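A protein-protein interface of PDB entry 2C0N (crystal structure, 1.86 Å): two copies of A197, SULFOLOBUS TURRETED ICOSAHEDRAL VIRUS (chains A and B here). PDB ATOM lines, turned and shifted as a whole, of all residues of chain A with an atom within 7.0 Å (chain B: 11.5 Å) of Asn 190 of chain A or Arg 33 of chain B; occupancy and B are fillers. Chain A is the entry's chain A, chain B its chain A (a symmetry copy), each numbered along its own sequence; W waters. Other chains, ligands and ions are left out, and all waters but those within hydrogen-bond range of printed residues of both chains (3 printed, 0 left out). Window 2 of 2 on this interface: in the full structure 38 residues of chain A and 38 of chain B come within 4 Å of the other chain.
O of Gly 11 of chain B sits at hydrogen-bond distance from N of Leu 15 of chain A (2.9 Å). NH1 of Arg 177 of chain A lies within hydrogen-bond range of O of Met 10 of chain B (3.1 Å). The side-chain hydroxyl (OG) of Ser 32 of chain B sits close to the backbone carbonyl oxygen (O) of Asn 190 of chain A (3.4 Å). O of Arg 33 of chain B sits at hydrogen-bond distance from ND2 of Asn 190 of chain A (3.4 Å). The side-chain amide nitrogen of Asn 190 of chain A sits close to the guanidinium group of Arg 34 of chain B, at 2.6 Å. The backbone carbonyl oxygen of Asp 191 of chain A is in hydrogen-bond range of the side-chain hydroxyl of Ser 32 of chain B, 2.4 Å away. A ring nitrogen (ND1) of His 192 of chain A sits at hydrogen-bond distance from the backbone NH (N) of Ser 32 of chain B (2.9 Å). A ring nitrogen (NE2) of His 192 of chain A lies close to the guanidinium group of Arg 34 of chain B (3.5 Å).
The side-chain carboxylate (OD2) of Asp 175 of chain A lies within salt-bridge range of the guanidinium group (NH2) of Arg 177 of chain A (3.6 Å). The guanidinium group (NH2) of Arg 177 of chain A lies within salt-bridge range of the side-chain carboxylate (OE1) of Glu 176 of chain A (3.3 Å). The backbone NH of Gln 189 of chain A sits at hydrogen-bond distance from the backbone carbonyl oxygen of Arg 177 of chain A (2.8 Å). N of Asp 191 of chain A sits at hydrogen-bond distance from OE1 of Gln 189 of chain A, 3.0 Å away. OG of Ser 9 of chain B lies within hydrogen-bond range of N of Gly 11 of chain B (3.0 Å). The side-chain amide nitrogen of Gln 40 of chain B lies within hydrogen-bond range of the backbone carbonyl oxygen of Leu 31 of chain B, 3.4 Å away.
Leu 15 of chain A touches Ser 9 of chain B. Leu 15 of chain A touches Ser 12 of chain B (CD1 to N, 3.8 Å). CG2 of Val 13 of chain B touches CD1 of Leu 15 of chain A (3.9 Å). CG2 of Ile 30 of chain B touches CD1 of Leu 15 of chain A, 3.7 Å away. Leu 15 of chain A touches Ser 32 of chain B (CD2 to OG, 3.2 Å). Glu 176 of chain A touches Met 10 of chain B. CB of Glu 176 of chain A touches O of Gly 11 of chain B, at 3.5 Å. Arg 33 of chain B touches Arg 177 of chain A. Ile 30 of chain B touches His 192 of chain A (O to CA, 3.4 Å). Ile 43 of chain B touches His 192 of chain A.
Asp 175 of chain A touches none of the printed residues of chain B. No residue of chain B comes within 4 Å of Leu 188 of chain A. No residue of chain B comes within 4 Å of Gln 189 of chain A. Asn 190 of chain A touches three residues of chain B. Printed residues of chain B within 4 Å of His 192 of chain A: Ile 30, Leu 31, Ser 32, Arg 34 and Ile 43. Pro 8 of chain B touches none of the printed residues of chain A. Of the printed residues of chain A, Leu 31 of chain B touches His 192. Printed residues of chain A within 4 Å of Arg 34 of chain B: Asn 190 (2.6 Å) and His 192 (3.3 Å). The nearest printed residue of chain A that does not touch Arg 33 of chain B is His 192 of chain A (5.7 Å).
No position is printed for both chains. Of the 19 pairs that touch across the chains among the printed residues, none has its exchanged pair printed and touching as well.
Water W3 bridges OE2 of Glu 176 of chain A (2.6 Å) and OG of Ser 12 of chain B (2.8 Å). Water W1 lies within hydrogen-bond range of O of Met 10 of chain B (2.7 Å), NH1 of Arg 33 of chain B (2.9 Å) and NH1 of Arg 177 of chain A (3.3 Å). Water W2 lies within hydrogen-bond range of the side-chain amide oxygen of Asn 190 of chain A (2.8 Å), the guanidinium group of Arg 177 of chain A (2.9 Å) and the backbone NH of Arg 33 of chain B (3.0 Å).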
ATOM      1  N   LEU A  15     -25.240   5.743  18.573  1.00  0.00           N
ATOM      2  CA  LEU A  15     -25.041   5.385  17.177  1.00  0.00           C
ATOM      3  C   LEU A  15     -25.868   6.196  16.205  1.00  0.00           C
ATOM      4  O   LEU A  15     -25.369   6.606  15.142  1.00  0.00           O
ATOM      5  CB  LEU A  15     -25.285   3.882  16.973  1.00  0.00           C
ATOM      6  CG  LEU A  15     -24.003   3.030  16.884  1.00  0.00           C
ATOM      7  CD1 LEU A  15     -23.089   3.159  18.104  1.00  0.00           C
ATOM      8  CD2 LEU A  15     -24.367   1.584  16.568  1.00  0.00           C
ATOM      9  N   PRO A  16     -27.146   6.364  16.499  1.00  0.00           N
ATOM     10  CA  PRO A  16     -27.954   7.165  15.547  1.00  0.00           C
ATOM     11  C   PRO A  16     -27.399   8.567  15.283  1.00  0.00           C
ATOM     12  O   PRO A  16     -27.515   9.051  14.155  1.00  0.00           O
ATOM     13  CB  PRO A  16     -29.335   7.182  16.211  1.00  0.00           C
ATOM     14  CG  PRO A  16     -29.323   5.931  17.073  1.00  0.00           C
ATOM     15  CD  PRO A  16     -27.973   5.805  17.587  1.00  0.00           C
ATOM     16  N   PHE A 173     -33.772  10.944  21.371  1.00  0.00           N
ATOM     17  CA  PHE A 173     -33.505   9.616  21.861  1.00  0.00           C
ATOM     18  C   PHE A 173     -33.549   9.507  23.351  1.00  0.00           C
ATOM     19  O   PHE A 173     -33.065  10.387  24.070  1.00  0.00           O
ATOM     20  CB  PHE A 173     -32.149   9.134  21.318  1.00  0.00           C
ATOM     21  CG  PHE A 173     -32.253   8.593  19.961  1.00  0.00           C
ATOM     22  CD1 PHE A 173     -32.264   9.430  18.843  1.00  0.00           C
ATOM     23  CD2 PHE A 173     -32.455   7.247  19.776  1.00  0.00           C
ATOM     24  CE1 PHE A 173     -32.438   8.913  17.558  1.00  0.00           C
ATOM     25  CE2 PHE A 173     -32.648   6.717  18.493  1.00  0.00           C
ATOM     26  CZ  PHE A 173     -32.639   7.569  17.361  1.00  0.00           C
ATOM     27  N   ASP A 175     -33.029   6.103  24.967  1.00  0.00           N
ATOM     28  CA  ASP A 175     -31.847   5.291  25.133  1.00  0.00           C
ATOM     29  C   ASP A 175     -31.103   5.297  23.813  1.00  0.00           C
ATOM     30  O   ASP A 175     -31.265   6.228  23.028  1.00  0.00           O
ATOM     31  CB  ASP A 175     -32.187   3.906  25.730  1.00  0.00           C
ATOM     32  CG  ASP A 175     -32.972   3.016  24.801  1.00  0.00           C
ATOM     33  OD1 ASP A 175     -33.176   3.430  23.666  1.00  0.00           O
ATOM     34  OD2 ASP A 175     -33.363   1.871  25.191  1.00  0.00           O
ATOM     35  N   GLU A 176     -30.263   4.297  23.570  1.00  0.00           N
ATOM     36  CA  GLU A 176     -29.471   4.275  22.355  1.00  0.00           C
ATOM     37  C   GLU A 176     -30.288   3.973  21.111  1.00  0.00           C
ATOM     38  O   GLU A 176     -29.798   4.203  20.005  1.00  0.00           O
ATOM     39  CB  GLU A 176     -28.359   3.252  22.493  1.00  0.00           C
ATOM     40  CG  GLU A 176     -27.403   3.564  23.592  1.00  0.00           C
ATOM     41  CD  GLU A 176     -27.797   3.076  24.979  1.00  0.00           C
ATOM     42  OE1 GLU A 176     -28.907   2.569  25.218  1.00  0.00           O
ATOM     43  OE2 GLU A 176     -26.931   3.186  25.859  1.00  0.00           O
ATOM     44  N   ARG A 177     -31.519   3.473  21.288  1.00  0.00           N
ATOM     45  CA  ARG A 177     -32.321   2.946  20.173  1.00  0.00           C
ATOM     46  C   ARG A 177     -33.732   3.524  20.064  1.00  0.00           C
ATOM     47  O   ARG A 177     -34.275   3.629  18.938  1.00  0.00           O
ATOM     48  CB  ARG A 177     -32.459   1.410  20.309  1.00  0.00           C
ATOM     49  CG  ARG A 177     -31.191   0.657  20.110  1.00  0.00           C
ATOM     50  CD  ARG A 177     -31.219  -0.788  20.753  1.00  0.00           C
ATOM     51  NE  ARG A 177     -31.278  -0.595  22.168  1.00  0.00           N
ATOM     52  CZ  ARG A 177     -30.260  -0.379  22.965  1.00  0.00           C
ATOM     53  NH1 ARG A 177     -28.972  -0.451  22.548  1.00  0.00           N
ATOM     54  NH2 ARG A 177     -30.523  -0.129  24.236  1.00  0.00           N
ATOM     55  N   LEU A 188     -37.910   3.202  16.878  1.00  0.00           N
ATOM     56  CA  LEU A 188     -36.747   2.406  17.241  1.00  0.00           C
ATOM     57  C   LEU A 188     -35.769   2.392  16.057  1.00  0.00           C
ATOM     58  O   LEU A 188     -36.152   2.042  14.959  1.00  0.00           O
ATOM     59  CB  LEU A 188     -37.223   1.012  17.586  1.00  0.00           C
ATOM     60  CG  LEU A 188     -36.353   0.053  18.393  1.00  0.00           C
ATOM     61  CD1 LEU A 188     -37.190  -1.082  18.900  1.00  0.00           C
ATOM     62  CD2 LEU A 188     -35.355  -0.515  17.451  1.00  0.00           C
ATOM     63  N   GLN A 189     -34.517   2.736  16.312  1.00  0.00           N
ATOM     64  CA  GLN A 189     -33.469   2.728  15.322  1.00  0.00           C
ATOM     65  C   GLN A 189     -32.354   1.842  15.832  1.00  0.00           C
ATOM     66  O   GLN A 189     -31.667   2.207  16.769  1.00  0.00           O
ATOM     67  CB  GLN A 189     -32.987   4.174  15.090  1.00  0.00           C
ATOM     68  CG  GLN A 189     -31.855   4.287  14.106  1.00  0.00           C
ATOM     69  CD  GLN A 189     -32.083   3.555  12.828  1.00  0.00           C
ATOM     70  OE1 GLN A 189     -31.625   2.404  12.644  1.00  0.00           O
ATOM     71  NE2 GLN A 189     -32.766   4.213  11.896  1.00  0.00           N
ATOM     72  N   ASN A 190     -32.157   0.676  15.231  1.00  0.00           N
ATOM     73  CA  ASN A 190     -31.146  -0.259  15.735  1.00  0.00           C
ATOM     74  C   ASN A 190     -30.215  -0.742  14.641  1.00  0.00           C
ATOM     75  O   ASN A 190     -29.675  -1.842  14.691  1.00  0.00           O
ATOM     76  CB  ASN A 190     -31.793  -1.431  16.492  1.00  0.00           C
ATOM     77  CG  ASN A 190     -30.809  -2.161  17.442  1.00  0.00           C
ATOM     78  OD1 ASN A 190     -30.000  -1.554  18.194  1.00  0.00           O
ATOM     79  ND2 ASN A 190     -30.892  -3.478  17.424  1.00  0.00           N
ATOM     80  N   ASP A 191     -29.972   0.114  13.665  1.00  0.00           N
ATOM     81  CA  ASP A 191     -29.056  -0.211  12.587  1.00  0.00           C
ATOM     82  C   ASP A 191     -27.605  -0.044  13.007  1.00  0.00           C
ATOM     83  O   ASP A 191     -27.275   0.750  13.901  1.00  0.00           O
ATOM     84  CB  ASP A 191     -29.308   0.708  11.400  1.00  0.00           C
ATOM     85  CG  ASP A 191     -30.559   0.355  10.631  1.00  0.00           C
ATOM     86  OD1 ASP A 191     -31.229  -0.663  10.952  1.00  0.00           O
ATOM     87  OD2 ASP A 191     -30.877   1.106   9.673  1.00  0.00           O
ATOM     88  N   HIS A 192     -26.733  -0.773  12.320  1.00  0.00           N
ATOM     89  CA  HIS A 192     -25.274  -0.569  12.435  1.00  0.00           C
ATOM     90  C   HIS A 192     -24.934   0.709  11.730  1.00  0.00           C
ATOM     91  O   HIS A 192     -25.718   1.217  10.916  1.00  0.00           O
ATOM     92  CB  HIS A 192     -24.537  -1.747  11.787  1.00  0.00           C
ATOM     93  CG  HIS A 192     -25.055  -3.085  12.203  1.00  0.00           C
ATOM     94  ND1 HIS A 192     -25.183  -3.464  13.528  1.00  0.00           N
ATOM     95  CD2 HIS A 192     -25.540  -4.109  11.468  1.00  0.00           C
ATOM     96  CE1 HIS A 192     -25.696  -4.682  13.578  1.00  0.00           C
ATOM     97  NE2 HIS A 192     -25.914  -5.101  12.341  1.00  0.00           N
ATOM     98  N   ILE B   7     -16.615  -2.814  15.216  1.00  0.00           N
ATOM     99  CA  ILE B   7     -16.644  -2.403  16.598  1.00  0.00           C
ATOM    100  C   ILE B   7     -17.979  -2.833  17.226  1.00  0.00           C
ATOM    101  O   ILE B   7     -18.983  -2.185  16.990  1.00  0.00           O
ATOM    102  CB  ILE B   7     -16.441  -0.873  16.696  1.00  0.00           C
ATOM    103  CG1 ILE B   7     -15.081  -0.471  16.091  1.00  0.00           C
ATOM    104  CG2 ILE B   7     -16.671  -0.428  18.185  1.00  0.00           C
ATOM    105  CD1 ILE B   7     -14.944   1.031  15.683  1.00  0.00           C
ATOM    106  N   PRO B   8     -17.997  -3.927  18.023  1.00  0.00           N
ATOM    107  CA  PRO B   8     -19.227  -4.361  18.708  1.00  0.00           C
ATOM    108  C   PRO B   8     -19.599  -3.312  19.738  1.00  0.00           C
ATOM    109  O   PRO B   8     -18.749  -2.955  20.550  1.00  0.00           O
ATOM    110  CB  PRO B   8     -18.805  -5.665  19.400  1.00  0.00           C
ATOM    111  CG  PRO B   8     -17.564  -6.058  18.807  1.00  0.00           C
ATOM    112  CD  PRO B   8     -16.894  -4.865  18.246  1.00  0.00           C
ATOM    113  N   SER B   9     -20.782  -2.748  19.651  1.00  0.00           N
ATOM    114  CA  SER B   9     -21.189  -1.772  20.669  1.00  0.00           C
ATOM    115  C   SER B   9     -22.445  -2.165  21.396  1.00  0.00           C
ATOM    116  O   SER B   9     -23.128  -3.112  20.994  1.00  0.00           O
ATOM    117  CB  SER B   9     -21.359  -0.403  20.025  1.00  0.00           C
ATOM    118  OG  SER B   9     -22.642  -0.285  19.526  1.00  0.00           O
ATOM    119  N   MET B  10     -22.766  -1.386  22.430  1.00  0.00           N
ATOM    120  CA  MET B  10     -24.065  -1.441  23.119  1.00  0.00           C
ATOM    121  C   MET B  10     -24.970  -0.270  22.736  1.00  0.00           C
ATOM    122  O   MET B  10     -25.984  -0.017  23.384  1.00  0.00           O
ATOM    123  CB  MET B  10     -23.865  -1.537  24.630  1.00  0.00           C
ATOM    124  CG  MET B  10     -22.876  -2.625  24.986  1.00  0.00           C
ATOM    125  SD  MET B  10     -23.832  -4.275  24.965  1.00  0.00           S
ATOM    126  CE  MET B  10     -24.543  -4.184  26.717  1.00  0.00           C
ATOM    127  N   GLY B  11     -24.626   0.402  21.618  1.00  0.00           N
ATOM    128  CA  GLY B  11     -25.432   1.478  21.061  1.00  0.00           C
ATOM    129  C   GLY B  11     -24.829   2.873  21.202  1.00  0.00           C
ATOM    130  O   GLY B  11     -25.410   3.857  20.733  1.00  0.00           O
ATOM    131  N   SER B  12     -23.661   2.968  21.823  1.00  0.00           N
ATOM    132  CA  SER B  12     -22.955   4.241  21.860  1.00  0.00           C
ATOM    133  C   SER B  12     -21.466   3.999  21.738  1.00  0.00           C
ATOM    134  O   SER B  12     -20.986   2.863  21.987  1.00  0.00           O
ATOM    135  CB  SER B  12     -23.272   4.993  23.121  1.00  0.00           C
ATOM    136  OG  SER B  12     -22.698   4.357  24.235  1.00  0.00           O
ATOM    137  N   VAL B  13     -20.743   5.070  21.386  1.00  0.00           N
ATOM    138  CA  VAL B  13     -19.290   5.037  21.321  1.00  0.00           C
ATOM    139  C   VAL B  13     -18.706   6.175  22.188  1.00  0.00           C
ATOM    140  O   VAL B  13     -19.074   7.340  22.021  1.00  0.00           O
ATOM    141  CB  VAL B  13     -18.797   5.194  19.891  1.00  0.00           C
ATOM    142  CG1 VAL B  13     -17.294   5.108  19.807  1.00  0.00           C
ATOM    143  CG2 VAL B  13     -19.384   4.058  19.027  1.00  0.00           C
ATOM    144  N   VAL B  29     -17.367  -0.408  10.723  1.00  0.00           N
ATOM    145  CA  VAL B  29     -18.743  -0.651  10.976  1.00  0.00           C
ATOM    146  C   VAL B  29     -18.905  -0.788  12.491  1.00  0.00           C
ATOM    147  O   VAL B  29     -18.285  -1.647  13.123  1.00  0.00           O
ATOM    148  CB  VAL B  29     -19.234  -1.917  10.318  1.00  0.00           C
ATOM    149  CG1 VAL B  29     -20.705  -2.163  10.656  1.00  0.00           C
ATOM    150  CG2 VAL B  29     -19.066  -1.839   8.797  1.00  0.00           C
ATOM    151  N   ILE B  30     -19.682   0.095  13.069  1.00  0.00           N
ATOM    152  CA  ILE B  30     -20.007  -0.008  14.472  1.00  0.00           C
ATOM    153  C   ILE B  30     -21.308  -0.800  14.556  1.00  0.00           C
ATOM    154  O   ILE B  30     -22.296  -0.417  13.966  1.00  0.00           O
ATOM    155  CB  ILE B  30     -20.225   1.352  15.136  1.00  0.00           C
ATOM    156  CG1 ILE B  30     -19.033   2.263  14.891  1.00  0.00           C
ATOM    157  CG2 ILE B  30     -20.350   1.161  16.642  1.00  0.00           C
ATOM    158  CD1 ILE B  30     -19.282   3.676  15.224  1.00  0.00           C
ATOM    159  N   LEU B  31     -21.290  -1.915  15.266  1.00  0.00           N
ATOM    160  CA  LEU B  31     -22.399  -2.839  15.274  1.00  0.00           C
ATOM    161  C   LEU B  31     -23.312  -2.465  16.423  1.00  0.00           C
ATOM    162  O   LEU B  31     -22.848  -2.331  17.571  1.00  0.00           O
ATOM    163  CB  LEU B  31     -21.891  -4.273  15.440  1.00  0.00           C
ATOM    164  CG  LEU B  31     -20.948  -4.693  14.293  1.00  0.00           C
ATOM    165  CD1 LEU B  31     -19.928  -5.693  14.730  1.00  0.00           C
ATOM    166  CD2 LEU B  31     -21.743  -5.204  13.184  1.00  0.00           C
ATOM    167  N   SER B  32     -24.600  -2.283  16.123  1.00  0.00           N
ATOM    168  CA  SER B  32     -25.622  -2.083  17.122  1.00  0.00           C
ATOM    169  C   SER B  32     -25.803  -3.311  17.970  1.00  0.00           C
ATOM    170  O   SER B  32     -25.334  -4.389  17.639  1.00  0.00           O
ATOM    171  CB  SER B  32     -26.956  -1.718  16.480  1.00  0.00           C
ATOM    172  OG  SER B  32     -26.848  -0.403  16.020  1.00  0.00           O
ATOM    173  N   ARG B  33     -26.474  -3.115  19.103  1.00  0.00           N
ATOM    174  CA  ARG B  33     -26.557  -4.126  20.102  1.00  0.00           C
ATOM    175  C   ARG B  33     -27.338  -5.305  19.539  1.00  0.00           C
ATOM    176  O   ARG B  33     -28.293  -5.115  18.812  1.00  0.00           O
ATOM    177  CB  ARG B  33     -27.276  -3.563  21.330  1.00  0.00           C
ATOM    178  CG  ARG B  33     -27.168  -4.436  22.502  1.00  0.00           C
ATOM    179  CD  ARG B  33     -27.724  -3.740  23.705  1.00  0.00           C
ATOM    180  NE  ARG B  33     -27.701  -4.636  24.852  1.00  0.00           N
ATOM    181  CZ  ARG B  33     -28.223  -4.366  26.041  1.00  0.00           C
ATOM    182  NH1 ARG B  33     -28.837  -3.205  26.268  1.00  0.00           N
ATOM    183  NH2 ARG B  33     -28.149  -5.284  27.016  1.00  0.00           N
ATOM    184  N   ARG B  34     -26.910  -6.516  19.836  1.00  0.00           N
ATOM    185  CA  ARG B  34     -27.712  -7.688  19.494  1.00  0.00           C
ATOM    186  C   ARG B  34     -27.856  -8.531  20.775  1.00  0.00           C
ATOM    187  O   ARG B  34     -27.527  -8.084  21.877  1.00  0.00           O
ATOM    188  CB  ARG B  34     -27.126  -8.467  18.291  1.00  0.00           C
ATOM    189  CG  ARG B  34     -27.096  -7.707  16.910  1.00  0.00           C
ATOM    190  CD  ARG B  34     -28.476  -7.518  16.266  1.00  0.00           C
ATOM    191  NE  ARG B  34     -28.598  -6.691  15.041  1.00  0.00           N
ATOM    192  CZ  ARG B  34     -28.870  -5.374  14.984  1.00  0.00           C
ATOM    193  NH1 ARG B  34     -28.948  -4.651  16.087  1.00  0.00           N
ATOM    194  NH2 ARG B  34     -29.019  -4.739  13.813  1.00  0.00           N
ATOM    195  N   ASN B  35     -28.356  -9.736  20.629  1.00  0.00           N
ATOM    196  CA  ASN B  35     -28.491 -10.659  21.740  1.00  0.00           C
ATOM    197  C   ASN B  35     -27.191 -10.880  22.522  1.00  0.00           C
ATOM    198  O   ASN B  35     -27.182 -11.005  23.741  1.00  0.00           O
ATOM    199  CB  ASN B  35     -29.029 -12.011  21.216  1.00  0.00           C
ATOM    200  CG  ASN B  35     -29.824 -11.860  19.892  1.00  0.00           C
ATOM    201  OD1 ASN B  35     -29.346 -11.255  18.907  1.00  0.00           O
ATOM    202  ND2 ASN B  35     -31.046 -12.390  19.881  1.00  0.00           N
ATOM    203  N   HIS B  36     -26.087 -10.948  21.803  1.00  0.00           N
ATOM    204  CA  HIS B  36     -24.830 -11.308  22.411  1.00  0.00           C
ATOM    205  C   HIS B  36     -23.727 -10.871  21.477  1.00  0.00           C
ATOM    206  O   HIS B  36     -23.940 -10.782  20.262  1.00  0.00           O
ATOM    207  CB  HIS B  36     -24.786 -12.818  22.641  1.00  0.00           C
ATOM    208  CG  HIS B  36     -23.520 -13.302  23.275  1.00  0.00           C
ATOM    209  ND1 HIS B  36     -23.424 -13.631  24.612  1.00  0.00           N
ATOM    210  CD2 HIS B  36     -22.310 -13.552  22.744  1.00  0.00           C
ATOM    211  CE1 HIS B  36     -22.191 -14.028  24.876  1.00  0.00           C
ATOM    212  NE2 HIS B  36     -21.488 -13.970  23.757  1.00  0.00           N
ATOM    213  N   VAL B  37     -22.548 -10.616  22.021  1.00  0.00           N
ATOM    214  CA  VAL B  37     -21.410 -10.169  21.185  1.00  0.00           C
ATOM    215  C   VAL B  37     -21.054 -11.180  20.085  1.00  0.00           C
ATOM    216  O   VAL B  37     -20.632 -10.819  18.995  1.00  0.00           O
ATOM    217  CB  VAL B  37     -20.175  -9.779  22.044  1.00  0.00           C
ATOM    218  CG1 VAL B  37     -19.625 -10.945  22.800  1.00  0.00           C
ATOM    219  CG2 VAL B  37     -19.105  -9.142  21.192  1.00  0.00           C
ATOM    220  N   ALA B  38     -21.245 -12.460  20.358  1.00  0.00           N
ATOM    221  CA  ALA B  38     -20.963 -13.481  19.351  1.00  0.00           C
ATOM    222  C   ALA B  38     -21.831 -13.294  18.110  1.00  0.00           C
ATOM    223  O   ALA B  38     -21.385 -13.528  16.982  1.00  0.00           O
ATOM    224  CB  ALA B  38     -21.107 -14.901  19.913  1.00  0.00           C
ATOM    225  N   VAL B  39     -23.069 -12.855  18.306  1.00  0.00           N
ATOM    226  CA  VAL B  39     -23.947 -12.600  17.176  1.00  0.00           C
ATOM    227  C   VAL B  39     -23.431 -11.404  16.397  1.00  0.00           C
ATOM    228  O   VAL B  39     -23.424 -11.401  15.168  1.00  0.00           O
ATOM    229  CB  VAL B  39     -25.390 -12.313  17.637  1.00  0.00           C
ATOM    230  CG1 VAL B  39     -26.271 -11.974  16.439  1.00  0.00           C
ATOM    231  CG2 VAL B  39     -25.966 -13.494  18.444  1.00  0.00           C
ATOM    232  N   GLN B  40     -22.976 -10.372  17.094  1.00  0.00           N
ATOM    233  CA  GLN B  40     -22.369  -9.220  16.389  1.00  0.00           C
ATOM    234  C   GLN B  40     -21.126  -9.624  15.615  1.00  0.00           C
ATOM    235  O   GLN B  40     -20.905  -9.162  14.494  1.00  0.00           O
ATOM    236  CB  GLN B  40     -22.009  -8.107  17.378  1.00  0.00           C
ATOM    237  CG  GLN B  40     -23.182  -7.523  18.123  1.00  0.00           C
ATOM    238  CD  GLN B  40     -22.743  -6.566  19.202  1.00  0.00           C
ATOM    239  OE1 GLN B  40     -22.068  -6.954  20.140  1.00  0.00           O
ATOM    240  NE2 GLN B  40     -23.139  -5.312  19.079  1.00  0.00           N
ATOM    241  N   ARG B  41     -20.286 -10.481  16.186  1.00  0.00           N
ATOM    242  CA  ARG B  41     -19.078 -10.904  15.480  1.00  0.00           C
ATOM    243  C   ARG B  41     -19.388 -11.745  14.249  1.00  0.00           C
ATOM    244  O   ARG B  41     -18.714 -11.647  13.234  1.00  0.00           O
ATOM    245  CB  ARG B  41     -18.118 -11.648  16.400  1.00  0.00           C
ATOM    246  CG  ARG B  41     -17.678 -10.854  17.574  1.00  0.00           C
ATOM    247  CD  ARG B  41     -16.455 -11.431  18.191  1.00  0.00           C
ATOM    248  NE  ARG B  41     -16.169 -10.855  19.501  1.00  0.00           N
ATOM    249  CZ  ARG B  41     -15.643  -9.659  19.694  1.00  0.00           C
ATOM    250  NH1 ARG B  41     -15.373  -8.877  18.667  1.00  0.00           N
ATOM    251  NH2 ARG B  41     -15.407  -9.222  20.926  1.00  0.00           N
ATOM    252  N   GLU B  42     -20.425 -12.556  14.309  1.00  0.00           N
ATOM    253  CA  GLU B  42     -20.826 -13.301  13.124  1.00  0.00           C
ATOM    254  C   GLU B  42     -21.359 -12.396  12.023  1.00  0.00           C
ATOM    255  O   GLU B  42     -21.098 -12.616  10.865  1.00  0.00           O
ATOM    256  CB  GLU B  42     -21.881 -14.335  13.479  1.00  0.00           C
ATOM    257  CG  GLU B  42     -22.009 -15.443  12.456  1.00  0.00           C
ATOM    258  CD  GLU B  42     -20.832 -16.354  12.485  1.00  0.00           C
ATOM    259  OE1 GLU B  42     -20.534 -16.895  13.555  1.00  0.00           O
ATOM    260  OE2 GLU B  42     -20.162 -16.482  11.455  1.00  0.00           O
ATOM    261  N   ILE B  43     -22.185 -11.419  12.380  1.00  0.00           N
ATOM    262  CA  ILE B  43     -22.660 -10.420  11.430  1.00  0.00           C
ATOM    263  C   ILE B  43     -21.471  -9.729  10.781  1.00  0.00           C
ATOM    264  O   ILE B  43     -21.427  -9.563   9.561  1.00  0.00           O
ATOM    265  CB  ILE B  43     -23.541  -9.382  12.154  1.00  0.00           C
ATOM    266  CG1 ILE B  43     -24.882 -10.008  12.521  1.00  0.00           C
ATOM    267  CG2 ILE B  43     -23.767  -8.104  11.295  1.00  0.00           C
ATOM    268  CD1 ILE B  43     -25.668  -9.212  13.495  1.00  0.00           C
ATOM    269  N   ALA B  44     -20.495  -9.337  11.600  1.00  0.00           N
ATOM    270  CA  ALA B  44     -19.264  -8.688  11.096  1.00  0.00           C
ATOM    271  C   ALA B  44     -18.581  -9.547  10.035  1.00  0.00           C
ATOM    272  O   ALA B  44     -18.294  -9.046   8.960  1.00  0.00           O
ATOM    273  CB  ALA B  44     -18.311  -8.420  12.205  1.00  0.00           C
ATOM    274  N   MET B  47     -20.624  -9.589   6.735  1.00  0.00           N
ATOM    275  CA  MET B  47     -20.468  -8.340   6.009  1.00  0.00           C
ATOM    276  C   MET B  47     -19.051  -8.249   5.395  1.00  0.00           C
ATOM    277  O   MET B  47     -18.897  -7.965   4.220  1.00  0.00           O
ATOM    278  CB  MET B  47     -20.704  -7.153   6.930  1.00  0.00           C
ATOM    279  CG  MET B  47     -22.187  -6.973   7.377  1.00  0.00           C
ATOM    280  SD  MET B  47     -22.303  -5.495   8.637  1.00  0.00           S
ATOM    281  CE  MET B  47     -21.775  -4.066   7.373  1.00  0.00           C
ATOM    282  N   GLU B  62     -15.562  -1.606  21.665  1.00  0.00           N
ATOM    283  CA  GLU B  62     -15.880  -0.182  21.793  1.00  0.00           C
ATOM    284  C   GLU B  62     -15.187   0.491  23.002  1.00  0.00           C
ATOM    285  O   GLU B  62     -15.104   1.712  23.081  1.00  0.00           O
ATOM    286  CB  GLU B  62     -17.385  -0.006  21.846  1.00  0.00           C
ATOM    287  CG  GLU B  62     -17.879   1.427  22.005  1.00  0.00           C
ATOM    288  CD  GLU B  62     -17.959   1.896  23.450  1.00  0.00           C
ATOM    289  OE1 GLU B  62     -18.058   1.023  24.350  1.00  0.00           O
ATOM    290  OE2 GLU B  62     -17.902   3.129  23.703  1.00  0.00           O
HETATM  291  O   HOH W   1     -27.474  -0.717  25.470  1.00  0.00           O
HETATM  292  O   HOH W   2     -27.929  -0.639  19.820  1.00  0.00           O
HETATM  293  O   HOH W   3     -24.725   4.512  26.091  1.00  0.00           O
